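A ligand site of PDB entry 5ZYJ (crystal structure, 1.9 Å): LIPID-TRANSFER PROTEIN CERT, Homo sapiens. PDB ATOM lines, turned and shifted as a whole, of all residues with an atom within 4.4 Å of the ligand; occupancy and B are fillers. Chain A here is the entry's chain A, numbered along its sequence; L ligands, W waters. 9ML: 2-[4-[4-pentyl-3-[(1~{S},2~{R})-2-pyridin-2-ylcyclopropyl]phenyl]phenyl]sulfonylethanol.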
ATOM      1  N   PHE A  75       6.083   8.512  -4.726  1.00  0.00           N
ATOM      2  CA  PHE A  75       5.005   9.361  -5.142  1.00  0.00           C
ATOM      3  C   PHE A  75       4.395   8.856  -6.472  1.00  0.00           C
ATOM      4  O   PHE A  75       3.168   8.906  -6.684  1.00  0.00           O
ATOM      5  CB  PHE A  75       5.487  10.868  -5.207  1.00  0.00           C
ATOM      6  CG  PHE A  75       4.372  11.854  -5.495  1.00  0.00           C
ATOM      7  CD1 PHE A  75       3.314  12.025  -4.579  1.00  0.00           C
ATOM      8  CD2 PHE A  75       4.421  12.676  -6.600  1.00  0.00           C
ATOM      9  CE1 PHE A  75       2.318  12.956  -4.852  1.00  0.00           C
ATOM     10  CE2 PHE A  75       3.444  13.611  -6.862  1.00  0.00           C
ATOM     11  CZ  PHE A  75       2.405  13.783  -5.972  1.00  0.00           C
ATOM     12  N   ARG A  81       0.157   3.492  -3.897  1.00  0.00           N
ATOM     13  CA  ARG A  81      -0.791   4.607  -3.721  1.00  0.00           C
ATOM     14  C   ARG A  81      -1.658   4.453  -2.497  1.00  0.00           C
ATOM     15  O   ARG A  81      -1.752   5.389  -1.727  1.00  0.00           O
ATOM     16  CB  ARG A  81      -1.721   4.726  -4.898  1.00  0.00           C
ATOM     17  CG  ARG A  81      -1.199   5.632  -5.928  1.00  0.00           C
ATOM     18  CD  ARG A  81      -1.188   7.116  -5.531  1.00  0.00           C
ATOM     19  NE  ARG A  81      -1.364   7.839  -6.773  1.00  0.00           N
ATOM     20  CZ  ARG A  81      -0.444   7.917  -7.709  1.00  0.00           C
ATOM     21  NH1 ARG A  81      -0.719   8.540  -8.822  1.00  0.00           N
ATOM     22  NH2 ARG A  81       0.736   7.376  -7.514  1.00  0.00           N
ATOM     23  N   TRP A  84      -0.526   5.416   1.140  1.00  0.00           N
ATOM     24  CA  TRP A  84      -0.391   6.781   1.682  1.00  0.00           C
ATOM     25  C   TRP A  84      -1.580   7.716   1.390  1.00  0.00           C
ATOM     26  O   TRP A  84      -1.832   8.662   2.171  1.00  0.00           O
ATOM     27  CB  TRP A  84       0.986   7.420   1.311  1.00  0.00           C
ATOM     28  CG  TRP A  84       1.253   7.485  -0.186  1.00  0.00           C
ATOM     29  CD1 TRP A  84       1.923   6.569  -0.957  1.00  0.00           C
ATOM     30  CD2 TRP A  84       0.847   8.529  -1.065  1.00  0.00           C
ATOM     31  NE1 TRP A  84       1.951   6.995  -2.313  1.00  0.00           N
ATOM     32  CE2 TRP A  84       1.309   8.194  -2.392  1.00  0.00           C
ATOM     33  CE3 TRP A  84       0.160   9.725  -0.879  1.00  0.00           C
ATOM     34  CZ2 TRP A  84       1.060   9.011  -3.489  1.00  0.00           C
ATOM     35  CZ3 TRP A  84      -0.123  10.527  -1.974  1.00  0.00           C
ATOM     36  CH2 TRP A  84       0.329  10.173  -3.265  1.00  0.00           C
ATOM     37  N   GLU A  85      -2.264   7.497   0.278  1.00  0.00           N
ATOM     38  CA  GLU A  85      -3.421   8.303  -0.144  1.00  0.00           C
ATOM     39  C   GLU A  85      -4.502   8.108   0.898  1.00  0.00           C
ATOM     40  O   GLU A  85      -4.724   6.970   1.282  1.00  0.00           O
ATOM     41  CB  GLU A  85      -3.995   7.752  -1.448  1.00  0.00           C
ATOM     42  CG  GLU A  85      -3.158   8.065  -2.681  1.00  0.00           C
ATOM     43  CD  GLU A  85      -3.359   9.492  -3.148  1.00  0.00           C
ATOM     44  OE1 GLU A  85      -3.487   9.692  -4.350  1.00  0.00           O
ATOM     45  OE2 GLU A  85      -3.396  10.404  -2.301  1.00  0.00           O
ATOM     46  N   THR A  87      -7.496  10.314   0.408  1.00  0.00           N
ATOM     47  CA  THR A  87      -8.645  11.023  -0.155  1.00  0.00           C
ATOM     48  C   THR A  87      -9.230  10.438  -1.441  1.00  0.00           C
ATOM     49  O   THR A  87     -10.172  10.992  -2.026  1.00  0.00           O
ATOM     50  CB  THR A  87      -8.368  12.549  -0.425  1.00  0.00           C
ATOM     51  OG1 THR A  87      -7.384  12.662  -1.446  1.00  0.00           O
ATOM     52  CG2 THR A  87      -7.854  13.335   0.835  1.00  0.00           C
ATOM     53  N   ILE A  88      -8.697   9.313  -1.883  1.00  0.00           N
ATOM     54  CA  ILE A  88      -9.055   8.671  -3.174  1.00  0.00           C
ATOM     55  C   ILE A  88     -10.106   7.579  -2.886  1.00  0.00           C
ATOM     56  O   ILE A  88      -9.882   6.746  -2.024  1.00  0.00           O
ATOM     57  CB  ILE A  88      -7.839   7.858  -3.599  1.00  0.00           C
ATOM     58  CG1 ILE A  88      -6.683   8.792  -3.854  1.00  0.00           C
ATOM     59  CG2 ILE A  88      -8.116   7.051  -4.858  1.00  0.00           C
ATOM     60  CD1 ILE A  88      -6.988   9.802  -4.927  1.00  0.00           C
ATOM     61  N   GLN A 106      -8.959   8.996 -11.467  1.00  0.00           N
ATOM     62  CA  GLN A 106      -9.233   8.670 -10.033  1.00  0.00           C
ATOM     63  C   GLN A 106     -10.382   9.491  -9.562  1.00  0.00           C
ATOM     64  O   GLN A 106     -10.673  10.566 -10.159  1.00  0.00           O
ATOM     65  CB  GLN A 106      -8.044   8.899  -9.106  1.00  0.00           C
ATOM     66  CG  GLN A 106      -7.642  10.417  -8.999  1.00  0.00           C
ATOM     67  CD  GLN A 106      -6.251  10.584  -8.365  1.00  0.00           C
ATOM     68  OE1 GLN A 106      -5.346   9.756  -8.608  1.00  0.00           O
ATOM     69  NE2 GLN A 106      -6.020  11.716  -7.645  1.00  0.00           N
ATOM     70  N   HIS A 108     -12.044  11.289  -6.079  1.00  0.00           N
ATOM     71  CA  HIS A 108     -11.830  11.618  -4.668  1.00  0.00           C
ATOM     72  C   HIS A 108     -13.060  11.428  -3.764  1.00  0.00           C
ATOM     73  O   HIS A 108     -14.179  11.576  -4.216  1.00  0.00           O
ATOM     74  CB  HIS A 108     -11.271  13.062  -4.534  1.00  0.00           C
ATOM     75  CG  HIS A 108      -9.875  13.186  -5.083  1.00  0.00           C
ATOM     76  ND1 HIS A 108      -8.758  13.037  -4.299  1.00  0.00           N
ATOM     77  CD2 HIS A 108      -9.423  13.310  -6.361  1.00  0.00           C
ATOM     78  CE1 HIS A 108      -7.658  13.141  -5.051  1.00  0.00           C
ATOM     79  NE2 HIS A 108      -8.047  13.297  -6.308  1.00  0.00           N
ATOM     80  N   VAL A 111     -16.443  15.547  -0.163  1.00  0.00           N
ATOM     81  CA  VAL A 111     -16.482  16.317   1.063  1.00  0.00           C
ATOM     82  C   VAL A 111     -17.840  17.092   1.066  1.00  0.00           C
ATOM     83  O   VAL A 111     -18.020  18.081   0.366  1.00  0.00           O
ATOM     84  CB  VAL A 111     -15.242  17.240   1.224  1.00  0.00           C
ATOM     85  CG1 VAL A 111     -15.115  18.203   0.050  1.00  0.00           C
ATOM     86  CG2 VAL A 111     -15.264  18.019   2.541  1.00  0.00           C
ATOM     87  N   ALA A 114     -20.106  19.376  -1.091  1.00  0.00           N
ATOM     88  CA  ALA A 114     -19.685  19.556  -2.480  1.00  0.00           C
ATOM     89  C   ALA A 114     -19.950  18.234  -3.231  1.00  0.00           C
ATOM     90  O   ALA A 114     -19.919  17.145  -2.644  1.00  0.00           O
ATOM     91  CB  ALA A 114     -18.220  19.891  -2.493  1.00  0.00           C
ATOM     92  N   SER A 115     -20.203  18.318  -4.517  1.00  0.00           N
ATOM     93  CA  SER A 115     -20.285  17.049  -5.245  1.00  0.00           C
ATOM     94  C   SER A 115     -18.893  16.420  -5.428  1.00  0.00           C
ATOM     95  O   SER A 115     -17.878  17.083  -5.271  1.00  0.00           O
ATOM     96  CB  SER A 115     -21.106  17.173  -6.531  1.00  0.00           C
ATOM     97  OG  SER A 115     -20.520  18.082  -7.381  1.00  0.00           O
ATOM     98  N   ARG A 117     -15.543  14.915  -6.996  1.00  0.00           N
ATOM     99  CA  ARG A 117     -14.644  15.251  -8.134  1.00  0.00           C
ATOM    100  C   ARG A 117     -13.916  13.983  -8.657  1.00  0.00           C
ATOM    101  O   ARG A 117     -13.464  13.117  -7.849  1.00  0.00           O
ATOM    102  CB  ARG A 117     -13.626  16.299  -7.670  1.00  0.00           C
ATOM    103  CG  ARG A 117     -14.031  17.761  -7.992  1.00  0.00           C
ATOM    104  CD  ARG A 117     -15.284  18.241  -7.218  1.00  0.00           C
ATOM    105  NE  ARG A 117     -15.673  19.542  -7.732  1.00  0.00           N
ATOM    106  CZ  ARG A 117     -16.776  20.181  -7.389  1.00  0.00           C
ATOM    107  NH1 ARG A 117     -17.607  19.661  -6.484  1.00  0.00           N
ATOM    108  NH2 ARG A 117     -17.007  21.336  -7.957  1.00  0.00           N
ATOM    109  N   VAL A 119     -10.689  13.078 -11.734  1.00  0.00           N
ATOM    110  CA  VAL A 119      -9.511  13.683 -12.358  1.00  0.00           C
ATOM    111  C   VAL A 119      -8.968  12.647 -13.411  1.00  0.00           C
ATOM    112  O   VAL A 119      -9.009  11.417 -13.155  1.00  0.00           O
ATOM    113  CB  VAL A 119      -8.364  13.899 -11.318  1.00  0.00           C
ATOM    114  CG1 VAL A 119      -7.326  15.004 -11.791  1.00  0.00           C
ATOM    115  CG2 VAL A 119      -8.935  14.316  -9.947  1.00  0.00           C
ATOM    116  N   TYR A 121      -5.357  12.445 -15.533  1.00  0.00           N
ATOM    117  CA  TYR A 121      -4.127  13.139 -15.634  1.00  0.00           C
ATOM    118  C   TYR A 121      -2.973  12.206 -16.058  1.00  0.00           C
ATOM    119  O   TYR A 121      -2.934  11.007 -15.779  1.00  0.00           O
ATOM    120  CB  TYR A 121      -3.802  13.786 -14.243  1.00  0.00           C
ATOM    121  CG  TYR A 121      -3.562  12.842 -13.145  1.00  0.00           C
ATOM    122  CD1 TYR A 121      -4.663  12.338 -12.418  1.00  0.00           C
ATOM    123  CD2 TYR A 121      -2.279  12.460 -12.748  1.00  0.00           C
ATOM    124  CE1 TYR A 121      -4.449  11.529 -11.347  1.00  0.00           C
ATOM    125  CE2 TYR A 121      -2.089  11.648 -11.620  1.00  0.00           C
ATOM    126  CZ  TYR A 121      -3.215  11.170 -10.954  1.00  0.00           C
ATOM    127  OH  TYR A 121      -3.123  10.323  -9.860  1.00  0.00           O
ATOM    128  N   ASN A 143       2.181  15.653 -12.441  1.00  0.00           N
ATOM    129  CA  ASN A 143       0.857  15.109 -12.727  1.00  0.00           C
ATOM    130  C   ASN A 143       0.004  16.217 -13.301  1.00  0.00           C
ATOM    131  O   ASN A 143      -0.286  17.191 -12.587  1.00  0.00           O
ATOM    132  CB  ASN A 143       0.225  14.596 -11.416  1.00  0.00           C
ATOM    133  CG  ASN A 143       0.994  13.459 -10.799  1.00  0.00           C
ATOM    134  OD1 ASN A 143       1.612  12.674 -11.518  1.00  0.00           O
ATOM    135  ND2 ASN A 143       0.928  13.303  -9.455  1.00  0.00           N
ATOM    136  N   ALA A 160     -12.294  17.645 -12.225  1.00  0.00           N
ATOM    137  CA  ALA A 160     -11.336  18.663 -11.810  1.00  0.00           C
ATOM    138  C   ALA A 160     -10.157  18.594 -12.763  1.00  0.00           C
ATOM    139  O   ALA A 160      -9.930  17.521 -13.377  1.00  0.00           O
ATOM    140  CB  ALA A 160     -10.872  18.321 -10.405  1.00  0.00           C
ATOM    141  N   ILE A 162      -5.903  19.436 -12.979  1.00  0.00           N
ATOM    142  CA  ILE A 162      -4.781  19.620 -12.052  1.00  0.00           C
ATOM    143  C   ILE A 162      -3.510  19.820 -12.796  1.00  0.00           C
ATOM    144  O   ILE A 162      -3.337  19.341 -13.959  1.00  0.00           O
ATOM    145  CB  ILE A 162      -4.629  18.462 -11.029  1.00  0.00           C
ATOM    146  CG1 ILE A 162      -3.971  17.189 -11.678  1.00  0.00           C
ATOM    147  CG2 ILE A 162      -5.968  18.187 -10.329  1.00  0.00           C
ATOM    148  CD1 ILE A 162      -3.757  16.021 -10.766  1.00  0.00           C
ATOM    149  N   VAL A 164       0.213  19.398 -10.963  1.00  0.00           N
ATOM    150  CA  VAL A 164       0.889  19.175  -9.673  1.00  0.00           C
ATOM    151  C   VAL A 164       2.322  18.805 -10.041  1.00  0.00           C
ATOM    152  O   VAL A 164       2.544  18.080 -11.029  1.00  0.00           O
ATOM    153  CB  VAL A 164       0.230  18.026  -8.888  1.00  0.00           C
ATOM    154  CG1 VAL A 164       1.094  17.573  -7.709  1.00  0.00           C
ATOM    155  CG2 VAL A 164      -1.205  18.481  -8.437  1.00  0.00           C
ATOM    156  N   TYR A 192       6.670  21.275  -3.481  1.00  0.00           N
ATOM    157  CA  TYR A 192       5.456  20.626  -3.967  1.00  0.00           C
ATOM    158  C   TYR A 192       4.499  21.735  -4.406  1.00  0.00           C
ATOM    159  O   TYR A 192       4.245  22.678  -3.639  1.00  0.00           O
ATOM    160  CB  TYR A 192       4.842  19.766  -2.874  1.00  0.00           C
ATOM    161  CG  TYR A 192       3.455  19.230  -3.209  1.00  0.00           C
ATOM    162  CD1 TYR A 192       3.307  18.084  -3.999  1.00  0.00           C
ATOM    163  CD2 TYR A 192       2.302  19.911  -2.808  1.00  0.00           C
ATOM    164  CE1 TYR A 192       2.036  17.584  -4.326  1.00  0.00           C
ATOM    165  CE2 TYR A 192       1.037  19.454  -3.153  1.00  0.00           C
ATOM    166  CZ  TYR A 192       0.902  18.282  -3.910  1.00  0.00           C
ATOM    167  OH  TYR A 192      -0.343  17.829  -4.245  1.00  0.00           O
ATOM    168  N   VAL A 196      -5.138  23.414  -8.876  1.00  0.00           N
ATOM    169  CA  VAL A 196      -6.305  22.539  -9.067  1.00  0.00           C
ATOM    170  C   VAL A 196      -7.464  23.416  -9.410  1.00  0.00           C
ATOM    171  O   VAL A 196      -7.773  24.416  -8.661  1.00  0.00           O
ATOM    172  CB  VAL A 196      -6.617  21.786  -7.741  1.00  0.00           C
ATOM    173  CG1 VAL A 196      -7.939  21.045  -7.893  1.00  0.00           C
ATOM    174  CG2 VAL A 196      -5.473  20.881  -7.426  1.00  0.00           C
ATOM    175  N   PRO A 198     -11.228  22.955  -9.522  1.00  0.00           N
ATOM    176  CA  PRO A 198     -12.173  21.888  -9.073  1.00  0.00           C
ATOM    177  C   PRO A 198     -13.389  21.699 -10.034  1.00  0.00           C
ATOM    178  O   PRO A 198     -14.172  20.759  -9.894  1.00  0.00           O
ATOM    179  CB  PRO A 198     -12.681  22.401  -7.677  1.00  0.00           C
ATOM    180  CG  PRO A 198     -12.409  23.879  -7.677  1.00  0.00           C
ATOM    181  CD  PRO A 198     -11.248  24.161  -8.665  1.00  0.00           C
ATOM    182  N   LEU A 207     -13.904  24.396  -0.355  1.00  0.00           N
ATOM    183  CA  LEU A 207     -12.635  24.196  -1.101  1.00  0.00           C
ATOM    184  C   LEU A 207     -11.492  24.605  -0.231  1.00  0.00           C
ATOM    185  O   LEU A 207     -10.505  23.880  -0.093  1.00  0.00           O
ATOM    186  CB  LEU A 207     -12.633  25.043  -2.381  1.00  0.00           C
ATOM    187  CG  LEU A 207     -13.698  24.482  -3.333  1.00  0.00           C
ATOM    188  CD1 LEU A 207     -13.935  25.367  -4.528  1.00  0.00           C
ATOM    189  CD2 LEU A 207     -13.309  23.096  -3.821  1.00  0.00           C
ATOM    190  N   VAL A 210     -10.812  22.365   2.808  1.00  0.00           N
ATOM    191  CA  VAL A 210     -10.274  21.025   2.438  1.00  0.00           C
ATOM    192  C   VAL A 210      -8.793  21.227   2.091  1.00  0.00           C
ATOM    193  O   VAL A 210      -7.952  20.500   2.609  1.00  0.00           O
ATOM    194  CB  VAL A 210     -11.016  20.457   1.233  1.00  0.00           C
ATOM    195  CG1 VAL A 210     -10.272  19.210   0.644  1.00  0.00           C
ATOM    196  CG2 VAL A 210     -12.505  20.155   1.568  1.00  0.00           C
ATOM    197  N   ALA A 211      -8.455  22.230   1.270  1.00  0.00           N
ATOM    198  CA  ALA A 211      -7.026  22.459   0.999  1.00  0.00           C
ATOM    199  C   ALA A 211      -6.236  22.629   2.318  1.00  0.00           C
ATOM    200  O   ALA A 211      -5.095  22.146   2.513  1.00  0.00           O
ATOM    201  CB  ALA A 211      -6.818  23.645   0.084  1.00  0.00           C
ATOM    202  N   GLU A 214      -6.070  19.206   4.109  1.00  0.00           N
ATOM    203  CA  GLU A 214      -5.595  18.000   3.453  1.00  0.00           C
ATOM    204  C   GLU A 214      -4.189  18.159   2.908  1.00  0.00           C
ATOM    205  O   GLU A 214      -3.471  17.172   2.838  1.00  0.00           O
ATOM    206  CB  GLU A 214      -6.505  17.531   2.328  1.00  0.00           C
ATOM    207  CG  GLU A 214      -7.901  17.009   2.705  1.00  0.00           C
ATOM    208  CD  GLU A 214      -7.887  15.936   3.806  1.00  0.00           C
ATOM    209  OE1 GLU A 214      -6.971  15.071   3.797  1.00  0.00           O
ATOM    210  OE2 GLU A 214      -8.803  15.947   4.668  1.00  0.00           O
ATOM    211  N   TYR A 215      -3.765  19.352   2.521  1.00  0.00           N
ATOM    212  CA  TYR A 215      -2.334  19.428   1.984  1.00  0.00           C
ATOM    213  C   TYR A 215      -1.253  19.151   3.032  1.00  0.00           C
ATOM    214  O   TYR A 215      -0.396  18.363   2.803  1.00  0.00           O
ATOM    215  CB  TYR A 215      -2.025  20.696   1.165  1.00  0.00           C
ATOM    216  CG  TYR A 215      -2.691  20.668  -0.223  1.00  0.00           C
ATOM    217  CD1 TYR A 215      -2.294  19.694  -1.243  1.00  0.00           C
ATOM    218  CD2 TYR A 215      -3.671  21.582  -0.539  1.00  0.00           C
ATOM    219  CE1 TYR A 215      -2.881  19.731  -2.505  1.00  0.00           C
ATOM    220  CE2 TYR A 215      -4.249  21.615  -1.786  1.00  0.00           C
ATOM    221  CZ  TYR A 215      -3.833  20.699  -2.779  1.00  0.00           C
ATOM    222  OH  TYR A 215      -4.485  20.828  -4.007  1.00  0.00           O
HETATM  223  C12 9ML L   1      -4.013  15.133  -7.218  1.00  0.00           C
HETATM  224  C13 9ML L   1      -8.474  19.960  -3.676  1.00  0.00           C
HETATM  225  C14 9ML L   1      -7.976  19.808  -2.240  1.00  0.00           C
HETATM  226  C15 9ML L   1      -6.270  16.114  -1.056  1.00  0.00           C
HETATM  227  C17 9ML L   1      -5.998  18.507  -1.329  1.00  0.00           C
HETATM  228  C18 9ML L   1      -7.349  18.574  -1.788  1.00  0.00           C
HETATM  229  C19 9ML L   1      -7.588  16.248  -1.537  1.00  0.00           C
HETATM  230  C20 9ML L   1      -1.372  12.906  -5.705  1.00  0.00           C
HETATM  231  N1  9ML L   1      -8.138  17.449  -1.906  1.00  0.00           N
HETATM  232  C5  9ML L   1      -7.104  18.237  -4.859  1.00  0.00           C
HETATM  233  C6  9ML L   1      -6.939  17.214  -5.820  1.00  0.00           C
HETATM  234  C7  9ML L   1      -3.118  15.304  -6.182  1.00  0.00           C
HETATM  235  C9  9ML L   1      -4.666  16.680  -4.940  1.00  0.00           C
HETATM  236  O1  9ML L   1      -0.589  15.371  -5.486  1.00  0.00           O
HETATM  237  S1  9ML L   1      -1.512  14.637  -6.334  1.00  0.00           S
HETATM  238  O2  9ML L   1      -1.290  14.655  -7.775  1.00  0.00           O
HETATM  239  C21 9ML L   1      -2.231  11.963  -6.567  1.00  0.00           C
HETATM  240  O3  9ML L   1      -3.598  11.958  -6.139  1.00  0.00           O
HETATM  241  C8  9ML L   1      -3.374  16.092  -5.041  1.00  0.00           C
HETATM  242  C10 9ML L   1      -5.612  16.533  -5.957  1.00  0.00           C
HETATM  243  C11 9ML L   1      -5.305  15.752  -7.072  1.00  0.00           C
HETATM  244  C4  9ML L   1      -8.356  18.888  -4.743  1.00  0.00           C
HETATM  245  C3  9ML L   1      -9.459  18.480  -5.525  1.00  0.00           C
HETATM  246  C24 9ML L   1     -10.800  19.182  -5.457  1.00  0.00           C
HETATM  247  C25 9ML L   1     -11.849  18.329  -4.702  1.00  0.00           C
HETATM  248  C26 9ML L   1     -13.079  19.239  -4.562  1.00  0.00           C
HETATM  249  C27 9ML L   1     -13.543  19.145  -3.120  1.00  0.00           C
HETATM  250  C28 9ML L   1     -15.018  19.538  -3.155  1.00  0.00           C
HETATM  251  C23 9ML L   1      -9.303  17.488  -6.492  1.00  0.00           C
HETATM  252  C1  9ML L   1      -8.041  16.833  -6.616  1.00  0.00           C
HETATM  253  C22 9ML L   1      -9.448  19.930  -2.544  1.00  0.00           C
HETATM  254  C16 9ML L   1      -5.484  17.277  -0.940  1.00  0.00           C
HETATM  255  O   HOH W   1      -4.182  12.791  -3.780  1.00  0.00           O
HETATM  256  O   HOH W   2      -8.502  23.415  -4.129  1.00  0.00           O
HETATM  257  O   HOH W   3     -10.943  16.313  -1.945  1.00  0.00           O
HETATM  258  O   HOH W   4     -16.285  16.651  -2.655  1.00  0.00           O
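O2 of the ligand sits at hydrogen-bond distance from ND2 of Asn 143. The side-chain amide nitrogen (NE2) of Gln 106 lies within hydrogen-bond range of an oxygen (O3) of the ligand. An oxygen (O3) of the ligand is in hydrogen-bond range of the side-chain carboxylate (OE1) of Glu 85. The side-chain hydroxyl (OH) of Tyr 192 is in hydrogen-bond range of an oxygen (O1) of the ligand (2.8 Å).
O of Asn 143 is in hydrogen-bond range of N of Val 164, 2.8 Å away. The guanidinium group (NH1) of Arg 81 sits at hydrogen-bond distance from the side-chain hydroxyl (OH) of Tyr 121. The side-chain amide nitrogen (NE2) of Gln 106 sits at hydrogen-bond distance from a ring nitrogen (NE2) of His 108, 2.9 Å away. OE1 of Gln 106 is in hydrogen-bond range of OH of Tyr 121, at 2.6 Å. O of Phe 75 is in hydrogen-bond range of NH2 of Arg 81 (3.0 Å). The backbone NH (N) of Gln 106 lies within hydrogen-bond range of the backbone carbonyl oxygen (O) of Val 119, at 3.0 Å. The backbone carbonyl oxygen (O) of Arg 117 sits at hydrogen-bond distance from the backbone NH (N) of His 108 (2.9 Å). OE1 of Glu 85 is in salt-bridge range of NE of Arg 81 (3.7 Å).
CZ of Phe 75 touches O1 of the ligand, at 3.4 Å. Thr 87 touches the ligand. NE2 of His 108 touches C1 of the ligand, 3.5 Å away. Val 111 touches the ligand (CG1 to C28, 3.5 Å). Ala 114 touches the ligand. Arg 117 touches the ligand. OH of Tyr 121 touches C21 of the ligand, 3.8 Å away. CD1 of Ile 162 touches C12 of the ligand, 3.7 Å away. Val 164 touches the ligand. CG1 of Val 196 touches C3 of the ligand (3.8 Å). Leu 207 touches the ligand. Val 210 touches the ligand. CB of Glu 214 touches C16 of the ligand (3.4 Å). Tyr 215 touches the ligand (CZ to C17, 3.4 Å).
Water W1 lies within hydrogen-bond range of an oxygen (O3) of the ligand and the side-chain carboxylate (OE2) of Glu 85.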
